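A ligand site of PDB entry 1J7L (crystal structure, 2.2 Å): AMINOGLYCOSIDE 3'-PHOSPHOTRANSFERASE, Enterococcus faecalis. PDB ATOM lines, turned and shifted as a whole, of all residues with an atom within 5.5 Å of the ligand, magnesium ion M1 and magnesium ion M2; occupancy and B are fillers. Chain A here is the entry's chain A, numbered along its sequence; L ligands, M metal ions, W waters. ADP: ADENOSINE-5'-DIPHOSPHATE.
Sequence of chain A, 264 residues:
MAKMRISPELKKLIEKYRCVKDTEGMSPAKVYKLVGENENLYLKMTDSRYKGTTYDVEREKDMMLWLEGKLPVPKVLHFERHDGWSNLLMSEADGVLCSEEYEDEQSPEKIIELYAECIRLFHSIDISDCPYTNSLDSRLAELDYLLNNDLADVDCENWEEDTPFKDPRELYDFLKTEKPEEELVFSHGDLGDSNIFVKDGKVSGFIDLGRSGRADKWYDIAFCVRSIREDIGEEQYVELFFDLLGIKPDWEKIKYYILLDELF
The side-chain amino group of Lys 44 lies within salt-bridge range of an oxygen (O1A) of the ligand, at 2.8 Å.
The backbone NH of Ala 93 lies within hydrogen-bond range of a nitrogen (N1) of the ligand (2.8 Å).
An oxygen (O2B) of the ligand is in hydrogen-bond range of the side-chain hydroxyl of Ser 27, at 2.6 Å.
N6 of the ligand is in hydrogen-bond range of SD of Met 90 (3.4 Å).
N6 of the ligand lies within hydrogen-bond range of O of Ser 91 (2.9 Å).
An oxygen (O3') of the ligand is in hydrogen-bond range of the backbone carbonyl oxygen of Ser 194.
An oxygen (O2B) of the ligand sits close to the backbone NH of Ser 27 (3.4 Å).
The backbone NH of Asp 208 sits close to the side-chain carboxylate of Glu 60 (3.4 Å).
The side-chain amide nitrogen of Asn 195 sits at hydrogen-bond distance from the backbone carbonyl oxygen of Asp 190 (2.9 Å).
The backbone carbonyl oxygen of Asn 195 sits at hydrogen-bond distance from the backbone NH of Ile 207, at 3.0 Å.
The backbone carbonyl oxygen of Val 31 lies within hydrogen-bond range of the backbone NH of Asp 22 (2.8 Å).
The side-chain amino group (NZ) of Lys 44 lies close to the side-chain carboxylate (OD1) of Asp 208 (3.2 Å).
The backbone NH (N) of Ala 29 lies close to the side-chain hydroxyl (OG) of Ser 27 (3.1 Å).
The backbone carbonyl oxygen (O) of Tyr 42 is in hydrogen-bond range of the backbone NH (N) of Met 90 (2.7 Å).
OD2 of Asp 22 sits close to N of Glu 24.
An oxygen (O4') of the ligand lies close to the side-chain carboxylate of Asp 22, at 3.3 Å.
OE1 of Glu 24 touches O3' of the ligand, at 3.7 Å.
Val 31 touches the ligand (CG2 to O3A, 3.5 Å).
CZ of Tyr 42 touches N3 of the ligand, 3.3 Å away.
Glu 92 touches the ligand.
Leu 97 touches the ligand.
Phe 197 touches the ligand.
Ile 207 touches the ligand (CD1 to C3', 3.6 Å).
Hydrophobic or aromatic side chains within 4 Å of the ligand: Val 31, Tyr 42, Met 90, Ala 93, Leu 97, Phe 197 and Ile 207.
Within 4 Å of the ligand: Asp 22, Glu 24, Ser 27, Val 31, Tyr 42, Lys 44, Met 90, Ser 91, Glu 92, Ala 93, Leu 97, Ser 194, Asn 195, Phe 197, Ile 207 and Asp 208.
Within 4 Å of magnesium ion M1: Asn 195 and Asp 208.
Merely in contact with magnesium ion M2: Asp 190 (3.9 Å).
Two residues have an atom within 4 Å of magnesium ion M2: Asp 190 and Asp 208.
Magnesium ion M1 is bound by an oxygen (O3B) of the ligand, the side-chain carboxylate of Asp 208, an oxygen (O2A) of the ligand, water W2, the side-chain amide oxygen of Asn 195 and water W3.
Magnesium ion M1 has six donor atoms within binding distance.
Magnesium ion M2 is bound by water W9 (1.9 Å), OD2 of Asp 208 (2.0 Å), water W7 (2.0 Å), O1B of the ligand (2.1 Å), water W5 (2.1 Å) and OD1 of Asp 208 (2.2 Å).
Magnesium ion M2 has six donor atoms within binding distance.
Water W2 lies within hydrogen-bond range of an oxygen (O3') of the ligand, the side-chain carboxylate of Glu 24 and the side-chain hydroxyl of Ser 194.
Water W3 lies within hydrogen-bond range of OD2 of Asp 190 (2.9 Å), ND2 of Asn 195 (2.9 Å) and OG of Ser 194 (3.3 Å).
Water W5 lies within hydrogen-bond range of the side-chain carboxylate (OD2) of Asp 190 (2.7 Å) and the guanidinium group (NH2) of Arg 211 (3.4 Å).
Water W4 lies within hydrogen-bond range of O2B of the ligand, O of Ala 29 and O of Ser 27.
Water W1 lies within hydrogen-bond range of an oxygen (O2') of the ligand (2.7 Å) and the side-chain hydroxyl of Tyr 42 (3.5 Å).
Water W8 bridges an oxygen (O1A) of the ligand (2.7 Å) and the side-chain sulfur of Met 90 (3.5 Å).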
ATOM      1  N   ASP A  22      17.758  -3.717   7.868  1.00  0.00           N
ATOM      2  CA  ASP A  22      18.139  -3.097   6.600  1.00  0.00           C
ATOM      3  C   ASP A  22      17.021  -2.131   6.213  1.00  0.00           C
ATOM      4  O   ASP A  22      15.838  -2.495   6.247  1.00  0.00           O
ATOM      5  CB  ASP A  22      18.314  -4.169   5.513  1.00  0.00           C
ATOM      6  CG  ASP A  22      18.629  -3.576   4.158  1.00  0.00           C
ATOM      7  OD1 ASP A  22      19.757  -3.051   3.972  1.00  0.00           O
ATOM      8  OD2 ASP A  22      17.761  -3.655   3.271  1.00  0.00           O
ATOM      9  N   GLU A  24      16.456  -0.660   3.172  1.00  0.00           N
ATOM     10  CA  GLU A  24      15.976  -0.739   1.797  1.00  0.00           C
ATOM     11  C   GLU A  24      14.523  -1.194   1.663  1.00  0.00           C
ATOM     12  O   GLU A  24      13.692  -0.482   1.091  1.00  0.00           O
ATOM     13  CB  GLU A  24      16.898  -1.609   0.954  1.00  0.00           C
ATOM     14  CG  GLU A  24      16.574  -1.582  -0.536  1.00  0.00           C
ATOM     15  CD  GLU A  24      17.639  -2.247  -1.388  1.00  0.00           C
ATOM     16  OE1 GLU A  24      18.835  -1.910  -1.229  1.00  0.00           O
ATOM     17  OE2 GLU A  24      17.288  -3.101  -2.229  1.00  0.00           O
ATOM     18  N   GLY A  25      14.214  -2.374   2.205  1.00  0.00           N
ATOM     19  CA  GLY A  25      12.859  -2.905   2.138  1.00  0.00           C
ATOM     20  C   GLY A  25      12.269  -2.905   0.741  1.00  0.00           C
ATOM     21  O   GLY A  25      11.109  -2.551   0.545  1.00  0.00           O
ATOM     22  N   MET A  26      13.077  -3.300  -0.248  1.00  0.00           N
ATOM     23  CA  MET A  26      12.638  -3.339  -1.643  1.00  0.00           C
ATOM     24  C   MET A  26      11.772  -4.561  -1.945  1.00  0.00           C
ATOM     25  O   MET A  26      11.172  -4.649  -3.017  1.00  0.00           O
ATOM     26  CB  MET A  26      13.854  -3.313  -2.584  1.00  0.00           C
ATOM     27  CG  MET A  26      13.762  -2.289  -3.704  1.00  0.00           C
ATOM     28  SD  MET A  26      14.198  -0.594  -3.204  1.00  0.00           S
ATOM     29  CE  MET A  26      12.576   0.092  -2.808  1.00  0.00           C
ATOM     30  N   SER A  27      11.740  -5.509  -1.017  1.00  0.00           N
ATOM     31  CA  SER A  27      10.947  -6.714  -1.197  1.00  0.00           C
ATOM     32  C   SER A  27      10.149  -6.987   0.076  1.00  0.00           C
ATOM     33  O   SER A  27      10.353  -6.317   1.092  1.00  0.00           O
ATOM     34  CB  SER A  27      11.872  -7.910  -1.508  1.00  0.00           C
ATOM     35  OG  SER A  27      12.376  -8.506  -0.329  1.00  0.00           O
ATOM     36  N   ALA A  29      10.414  -9.272   1.983  1.00  0.00           N
ATOM     37  CA  ALA A  29      11.285  -9.931   2.958  1.00  0.00           C
ATOM     38  C   ALA A  29      11.777  -8.933   3.989  1.00  0.00           C
ATOM     39  O   ALA A  29      11.882  -7.731   3.702  1.00  0.00           O
ATOM     40  CB  ALA A  29      12.463 -10.575   2.261  1.00  0.00           C
ATOM     41  N   VAL A  31      14.894  -7.953   6.229  1.00  0.00           N
ATOM     42  CA  VAL A  31      16.330  -8.179   6.227  1.00  0.00           C
ATOM     43  C   VAL A  31      16.972  -7.527   7.433  1.00  0.00           C
ATOM     44  O   VAL A  31      16.719  -6.363   7.741  1.00  0.00           O
ATOM     45  CB  VAL A  31      16.985  -7.658   4.926  1.00  0.00           C
ATOM     46  CG1 VAL A  31      18.500  -7.868   4.978  1.00  0.00           C
ATOM     47  CG2 VAL A  31      16.412  -8.372   3.715  1.00  0.00           C
ATOM     48  N   TYR A  42      23.735 -11.922   8.364  1.00  0.00           N
ATOM     49  CA  TYR A  42      22.507 -11.387   7.835  1.00  0.00           C
ATOM     50  C   TYR A  42      21.403 -12.421   7.967  1.00  0.00           C
ATOM     51  O   TYR A  42      21.625 -13.622   7.790  1.00  0.00           O
ATOM     52  CB  TYR A  42      22.673 -10.937   6.376  1.00  0.00           C
ATOM     53  CG  TYR A  42      23.239  -9.541   6.254  1.00  0.00           C
ATOM     54  CD1 TYR A  42      24.612  -9.306   6.321  1.00  0.00           C
ATOM     55  CD2 TYR A  42      22.392  -8.449   6.075  1.00  0.00           C
ATOM     56  CE1 TYR A  42      25.122  -8.019   6.184  1.00  0.00           C
ATOM     57  CE2 TYR A  42      22.894  -7.160   5.932  1.00  0.00           C
ATOM     58  CZ  TYR A  42      24.259  -6.945   5.986  1.00  0.00           C
ATOM     59  OH  TYR A  42      24.752  -5.668   5.820  1.00  0.00           O
ATOM     60  N   LYS A  44      17.557 -13.076   6.730  1.00  0.00           N
ATOM     61  CA  LYS A  44      16.516 -12.688   5.791  1.00  0.00           C
ATOM     62  C   LYS A  44      15.310 -13.574   6.097  1.00  0.00           C
ATOM     63  O   LYS A  44      15.439 -14.789   6.208  1.00  0.00           O
ATOM     64  CB  LYS A  44      16.984 -12.899   4.363  1.00  0.00           C
ATOM     65  CG  LYS A  44      16.081 -12.239   3.333  1.00  0.00           C
ATOM     66  CD  LYS A  44      16.656 -12.317   1.931  1.00  0.00           C
ATOM     67  CE  LYS A  44      15.920 -11.364   0.999  1.00  0.00           C
ATOM     68  NZ  LYS A  44      16.482 -11.402  -0.377  1.00  0.00           N
ATOM     69  N   GLU A  60      15.980 -19.115  -1.643  1.00  0.00           N
ATOM     70  CA  GLU A  60      16.955 -18.377  -1.776  1.00  0.00           C
ATOM     71  C   GLU A  60      18.344 -19.443  -1.033  1.00  0.00           C
ATOM     72  O   GLU A  60      19.446 -19.588  -1.541  1.00  0.00           O
ATOM     73  CB  GLU A  60      16.763 -17.042  -1.100  1.00  0.00           C
ATOM     74  CG  GLU A  60      17.765 -16.173  -1.042  1.00  0.00           C
ATOM     75  CD  GLU A  60      17.334 -14.615  -0.646  1.00  0.00           C
ATOM     76  OE1 GLU A  60      16.372 -14.243  -0.106  1.00  0.00           O
ATOM     77  OE2 GLU A  60      17.973 -13.776  -0.892  1.00  0.00           O
ATOM     78  N   PRO A  74      27.041 -15.954  -0.121  1.00  0.00           N
ATOM     79  CA  PRO A  74      27.256 -16.077   1.327  1.00  0.00           C
ATOM     80  C   PRO A  74      27.062 -17.512   1.801  1.00  0.00           C
ATOM     81  O   PRO A  74      26.472 -18.342   1.100  1.00  0.00           O
ATOM     82  CB  PRO A  74      26.207 -15.129   1.920  1.00  0.00           C
ATOM     83  CG  PRO A  74      25.149 -15.064   0.874  1.00  0.00           C
ATOM     84  CD  PRO A  74      25.930 -15.020  -0.402  1.00  0.00           C
ATOM     85  N   MET A  90      22.710 -16.038   7.246  1.00  0.00           N
ATOM     86  CA  MET A  90      23.843 -16.203   6.340  1.00  0.00           C
ATOM     87  C   MET A  90      25.011 -15.313   6.727  1.00  0.00           C
ATOM     88  O   MET A  90      24.871 -14.378   7.517  1.00  0.00           O
ATOM     89  CB  MET A  90      23.404 -15.862   4.905  1.00  0.00           C
ATOM     90  CG  MET A  90      23.176 -14.365   4.682  1.00  0.00           C
ATOM     91  SD  MET A  90      22.155 -13.971   3.228  1.00  0.00           S
ATOM     92  CE  MET A  90      20.558 -13.826   4.006  1.00  0.00           C
ATOM     93  N   SER A  91      26.180 -15.598   6.162  1.00  0.00           N
ATOM     94  CA  SER A  91      27.362 -14.799   6.412  1.00  0.00           C
ATOM     95  C   SER A  91      27.254 -13.518   5.589  1.00  0.00           C
ATOM     96  O   SER A  91      26.408 -13.413   4.683  1.00  0.00           O
ATOM     97  CB  SER A  91      28.610 -15.565   6.002  1.00  0.00           C
ATOM     98  OG  SER A  91      28.585 -15.870   4.613  1.00  0.00           O
ATOM     99  N   GLU A  92      28.085 -12.542   5.920  1.00  0.00           N
ATOM    100  CA  GLU A  92      28.104 -11.280   5.207  1.00  0.00           C
ATOM    101  C   GLU A  92      28.842 -11.487   3.890  1.00  0.00           C
ATOM    102  O   GLU A  92      29.881 -12.144   3.842  1.00  0.00           O
ATOM    103  CB  GLU A  92      28.815 -10.211   6.042  1.00  0.00           C
ATOM    104  CG  GLU A  92      28.840  -8.834   5.403  1.00  0.00           C
ATOM    105  CD  GLU A  92      29.373  -7.765   6.333  1.00  0.00           C
ATOM    106  OE1 GLU A  92      30.545  -7.862   6.746  1.00  0.00           O
ATOM    107  OE2 GLU A  92      28.614  -6.823   6.657  1.00  0.00           O
ATOM    108  N   ALA A  93      28.283 -10.957   2.801  1.00  0.00           N
ATOM    109  CA  ALA A  93      28.909 -11.085   1.496  1.00  0.00           C
ATOM    110  C   ALA A  93      30.297 -10.445   1.511  1.00  0.00           C
ATOM    111  O   ALA A  93      30.542  -9.470   2.231  1.00  0.00           O
ATOM    112  CB  ALA A  93      28.042 -10.441   0.435  1.00  0.00           C
ATOM    113  N   LEU A  97      29.485  -3.532  -1.751  1.00  0.00           N
ATOM    114  CA  LEU A  97      28.229  -3.485  -2.484  1.00  0.00           C
ATOM    115  C   LEU A  97      28.450  -2.598  -3.707  1.00  0.00           C
ATOM    116  O   LEU A  97      29.048  -1.518  -3.589  1.00  0.00           O
ATOM    117  CB  LEU A  97      27.153  -2.875  -1.575  1.00  0.00           C
ATOM    118  CG  LEU A  97      25.682  -2.922  -1.983  1.00  0.00           C
ATOM    119  CD1 LEU A  97      25.229  -4.360  -2.094  1.00  0.00           C
ATOM    120  CD2 LEU A  97      24.853  -2.187  -0.932  1.00  0.00           C
ATOM    121  N   ASP A 190      17.607 -11.031 -10.369  1.00  0.00           N
ATOM    122  CA  ASP A 190      17.510  -9.637  -9.970  1.00  0.00           C
ATOM    123  C   ASP A 190      18.920  -9.084  -9.928  1.00  0.00           C
ATOM    124  O   ASP A 190      19.453  -8.753  -8.877  1.00  0.00           O
ATOM    125  CB  ASP A 190      16.816  -9.493  -8.614  1.00  0.00           C
ATOM    126  CG  ASP A 190      16.571  -8.040  -8.229  1.00  0.00           C
ATOM    127  OD1 ASP A 190      16.555  -7.190  -9.148  1.00  0.00           O
ATOM    128  OD2 ASP A 190      16.398  -7.735  -7.032  1.00  0.00           O
ATOM    129  N   SER A 194      22.481  -3.546  -5.980  1.00  0.00           N
ATOM    130  CA  SER A 194      22.261  -3.719  -4.548  1.00  0.00           C
ATOM    131  C   SER A 194      22.329  -5.191  -4.166  1.00  0.00           C
ATOM    132  O   SER A 194      22.208  -5.534  -2.989  1.00  0.00           O
ATOM    133  CB  SER A 194      20.893  -3.149  -4.151  1.00  0.00           C
ATOM    134  OG  SER A 194      19.846  -3.863  -4.807  1.00  0.00           O
ATOM    135  N   ASN A 195      22.505  -6.060  -5.163  1.00  0.00           N
ATOM    136  CA  ASN A 195      22.587  -7.513  -4.930  1.00  0.00           C
ATOM    137  C   ASN A 195      23.920  -8.082  -5.365  1.00  0.00           C
ATOM    138  O   ASN A 195      24.128  -9.295  -5.328  1.00  0.00           O
ATOM    139  CB  ASN A 195      21.472  -8.246  -5.685  1.00  0.00           C
ATOM    140  CG  ASN A 195      20.080  -7.808  -5.253  1.00  0.00           C
ATOM    141  OD1 ASN A 195      19.861  -7.403  -4.114  1.00  0.00           O
ATOM    142  ND2 ASN A 195      19.125  -7.908  -6.172  1.00  0.00           N
ATOM    143  N   PHE A 197      28.301  -7.671  -5.179  1.00  0.00           N
ATOM    144  CA  PHE A 197      29.436  -7.133  -4.442  1.00  0.00           C
ATOM    145  C   PHE A 197      30.697  -7.192  -5.291  1.00  0.00           C
ATOM    146  O   PHE A 197      30.886  -8.125  -6.060  1.00  0.00           O
ATOM    147  CB  PHE A 197      29.643  -7.918  -3.136  1.00  0.00           C
ATOM    148  CG  PHE A 197      28.525  -7.729  -2.149  1.00  0.00           C
ATOM    149  CD1 PHE A 197      27.311  -8.389  -2.322  1.00  0.00           C
ATOM    150  CD2 PHE A 197      28.682  -6.894  -1.046  1.00  0.00           C
ATOM    151  CE1 PHE A 197      26.268  -8.204  -1.421  1.00  0.00           C
ATOM    152  CE2 PHE A 197      27.652  -6.704  -0.144  1.00  0.00           C
ATOM    153  CZ  PHE A 197      26.431  -7.363  -0.324  1.00  0.00           C
ATOM    154  N   ILE A 207      23.822 -11.935  -3.848  1.00  0.00           N
ATOM    155  CA  ILE A 207      22.797 -12.185  -2.834  1.00  0.00           C
ATOM    156  C   ILE A 207      21.438 -11.981  -3.498  1.00  0.00           C
ATOM    157  O   ILE A 207      21.363 -11.647  -4.686  1.00  0.00           O
ATOM    158  CB  ILE A 207      22.913 -11.210  -1.645  1.00  0.00           C
ATOM    159  CG1 ILE A 207      22.804  -9.763  -2.140  1.00  0.00           C
ATOM    160  CG2 ILE A 207      24.201 -11.455  -0.883  1.00  0.00           C
ATOM    161  CD1 ILE A 207      22.830  -8.734  -1.018  1.00  0.00           C
ATOM    162  N   ASP A 208      20.368 -12.182  -2.726  1.00  0.00           N
ATOM    163  CA  ASP A 208      19.003 -12.028  -3.227  1.00  0.00           C
ATOM    164  C   ASP A 208      18.867 -13.029  -4.371  1.00  0.00           C
ATOM    165  O   ASP A 208      18.738 -12.645  -5.531  1.00  0.00           O
ATOM    166  CB  ASP A 208      18.797 -10.587  -3.708  1.00  0.00           C
ATOM    167  CG  ASP A 208      17.359 -10.134  -3.651  1.00  0.00           C
ATOM    168  OD1 ASP A 208      16.457 -10.985  -3.556  1.00  0.00           O
ATOM    169  OD2 ASP A 208      17.145  -8.919  -3.712  1.00  0.00           O
ATOM    170  N   ARG A 211      14.984 -15.634  -7.100  1.00  0.00           N
ATOM    171  CA  ARG A 211      14.595 -15.875  -8.488  1.00  0.00           C
ATOM    172  C   ARG A 211      15.702 -16.552  -9.283  1.00  0.00           C
ATOM    173  O   ARG A 211      15.613 -16.681 -10.501  1.00  0.00           O
ATOM    174  CB  ARG A 211      14.201 -14.559  -9.192  1.00  0.00           C
ATOM    175  CG  ARG A 211      12.862 -13.974  -8.747  1.00  0.00           C
ATOM    176  CD  ARG A 211      12.530 -12.688  -9.486  1.00  0.00           C
ATOM    177  NE  ARG A 211      12.119 -11.649  -8.541  1.00  0.00           N
ATOM    178  CZ  ARG A 211      12.591 -10.405  -8.524  1.00  0.00           C
ATOM    179  NH1 ARG A 211      13.503 -10.024  -9.417  1.00  0.00           N
ATOM    180  NH2 ARG A 211      12.161  -9.551  -7.613  1.00  0.00           N
HETATM  181  PB  ADP L   1      15.658  -7.928  -0.880  1.00  0.00           P
HETATM  182  O1B ADP L   1      15.248  -9.146  -1.623  1.00  0.00           O
HETATM  183  O2B ADP L   1      14.638  -7.141  -0.166  1.00  0.00           O
HETATM  184  O3B ADP L   1      16.409  -6.914  -1.896  1.00  0.00           O
HETATM  185  PA  ADP L   1      18.389  -8.503  -0.112  1.00  0.00           P
HETATM  186  O1A ADP L   1      18.757  -9.918   0.099  1.00  0.00           O
HETATM  187  O2A ADP L   1      18.696  -7.849  -1.394  1.00  0.00           O
HETATM  188  O3A ADP L   1      16.810  -8.330   0.191  1.00  0.00           O
HETATM  189  O5' ADP L   1      19.053  -7.659   1.064  1.00  0.00           O
HETATM  190  C5' ADP L   1      18.749  -6.269   1.219  1.00  0.00           C
HETATM  191  C4' ADP L   1      20.048  -5.484   1.363  1.00  0.00           C
HETATM  192  O4' ADP L   1      20.705  -5.850   2.575  1.00  0.00           O
HETATM  193  C3' ADP L   1      21.078  -5.825   0.277  1.00  0.00           C
HETATM  194  O3' ADP L   1      20.986  -4.853  -0.766  1.00  0.00           O
HETATM  195  C2' ADP L   1      22.384  -5.645   1.052  1.00  0.00           C
HETATM  196  O2' ADP L   1      22.669  -4.244   1.189  1.00  0.00           O
HETATM  197  C1' ADP L   1      22.090  -6.193   2.443  1.00  0.00           C
HETATM  198  N9  ADP L   1      22.391  -7.621   2.619  1.00  0.00           N
HETATM  199  C8  ADP L   1      21.537  -8.688   2.687  1.00  0.00           C
HETATM  200  N7  ADP L   1      22.128  -9.832   2.850  1.00  0.00           N
HETATM  201  C5  ADP L   1      23.474  -9.517   2.878  1.00  0.00           C
HETATM  202  C6  ADP L   1      24.656 -10.300   3.030  1.00  0.00           C
HETATM  203  N6  ADP L   1      24.636 -11.624   3.170  1.00  0.00           N
HETATM  204  N1  ADP L   1      25.837  -9.652   3.021  1.00  0.00           N
HETATM  205  C2  ADP L   1      25.857  -8.320   2.869  1.00  0.00           C
HETATM  206  N3  ADP L   1      24.827  -7.481   2.729  1.00  0.00           N
HETATM  207  C4  ADP L   1      23.649  -8.167   2.739  1.00  0.00           C
HETATM  208 MG    MG M   1      17.977  -7.121  -3.185  1.00  0.00          MG
HETATM  209 MG    MG M   2      15.128  -9.224  -3.684  1.00  0.00          MG
HETATM  210  O   HOH W   1      24.971  -4.431   2.574  1.00  0.00           O
HETATM  211  O   HOH W   2      18.907  -5.378  -2.491  1.00  0.00           O
HETATM  212  O   HOH W   3      17.300  -6.002  -4.937  1.00  0.00           O
HETATM  213  O   HOH W   4      13.403  -6.077   1.969  1.00  0.00           O
HETATM  214  O   HOH W   5      14.986  -9.662  -5.766  1.00  0.00           O
HETATM  215  O   HOH W   6      12.448 -11.160  -1.088  1.00  0.00           O
HETATM  216  O   HOH W   7      13.585 -10.562  -3.546  1.00  0.00           O
HETATM  217  O   HOH W   8      20.302 -11.533   1.629  1.00  0.00           O
HETATM  218  O   HOH W   9      14.432  -7.441  -3.878  1.00  0.00           O
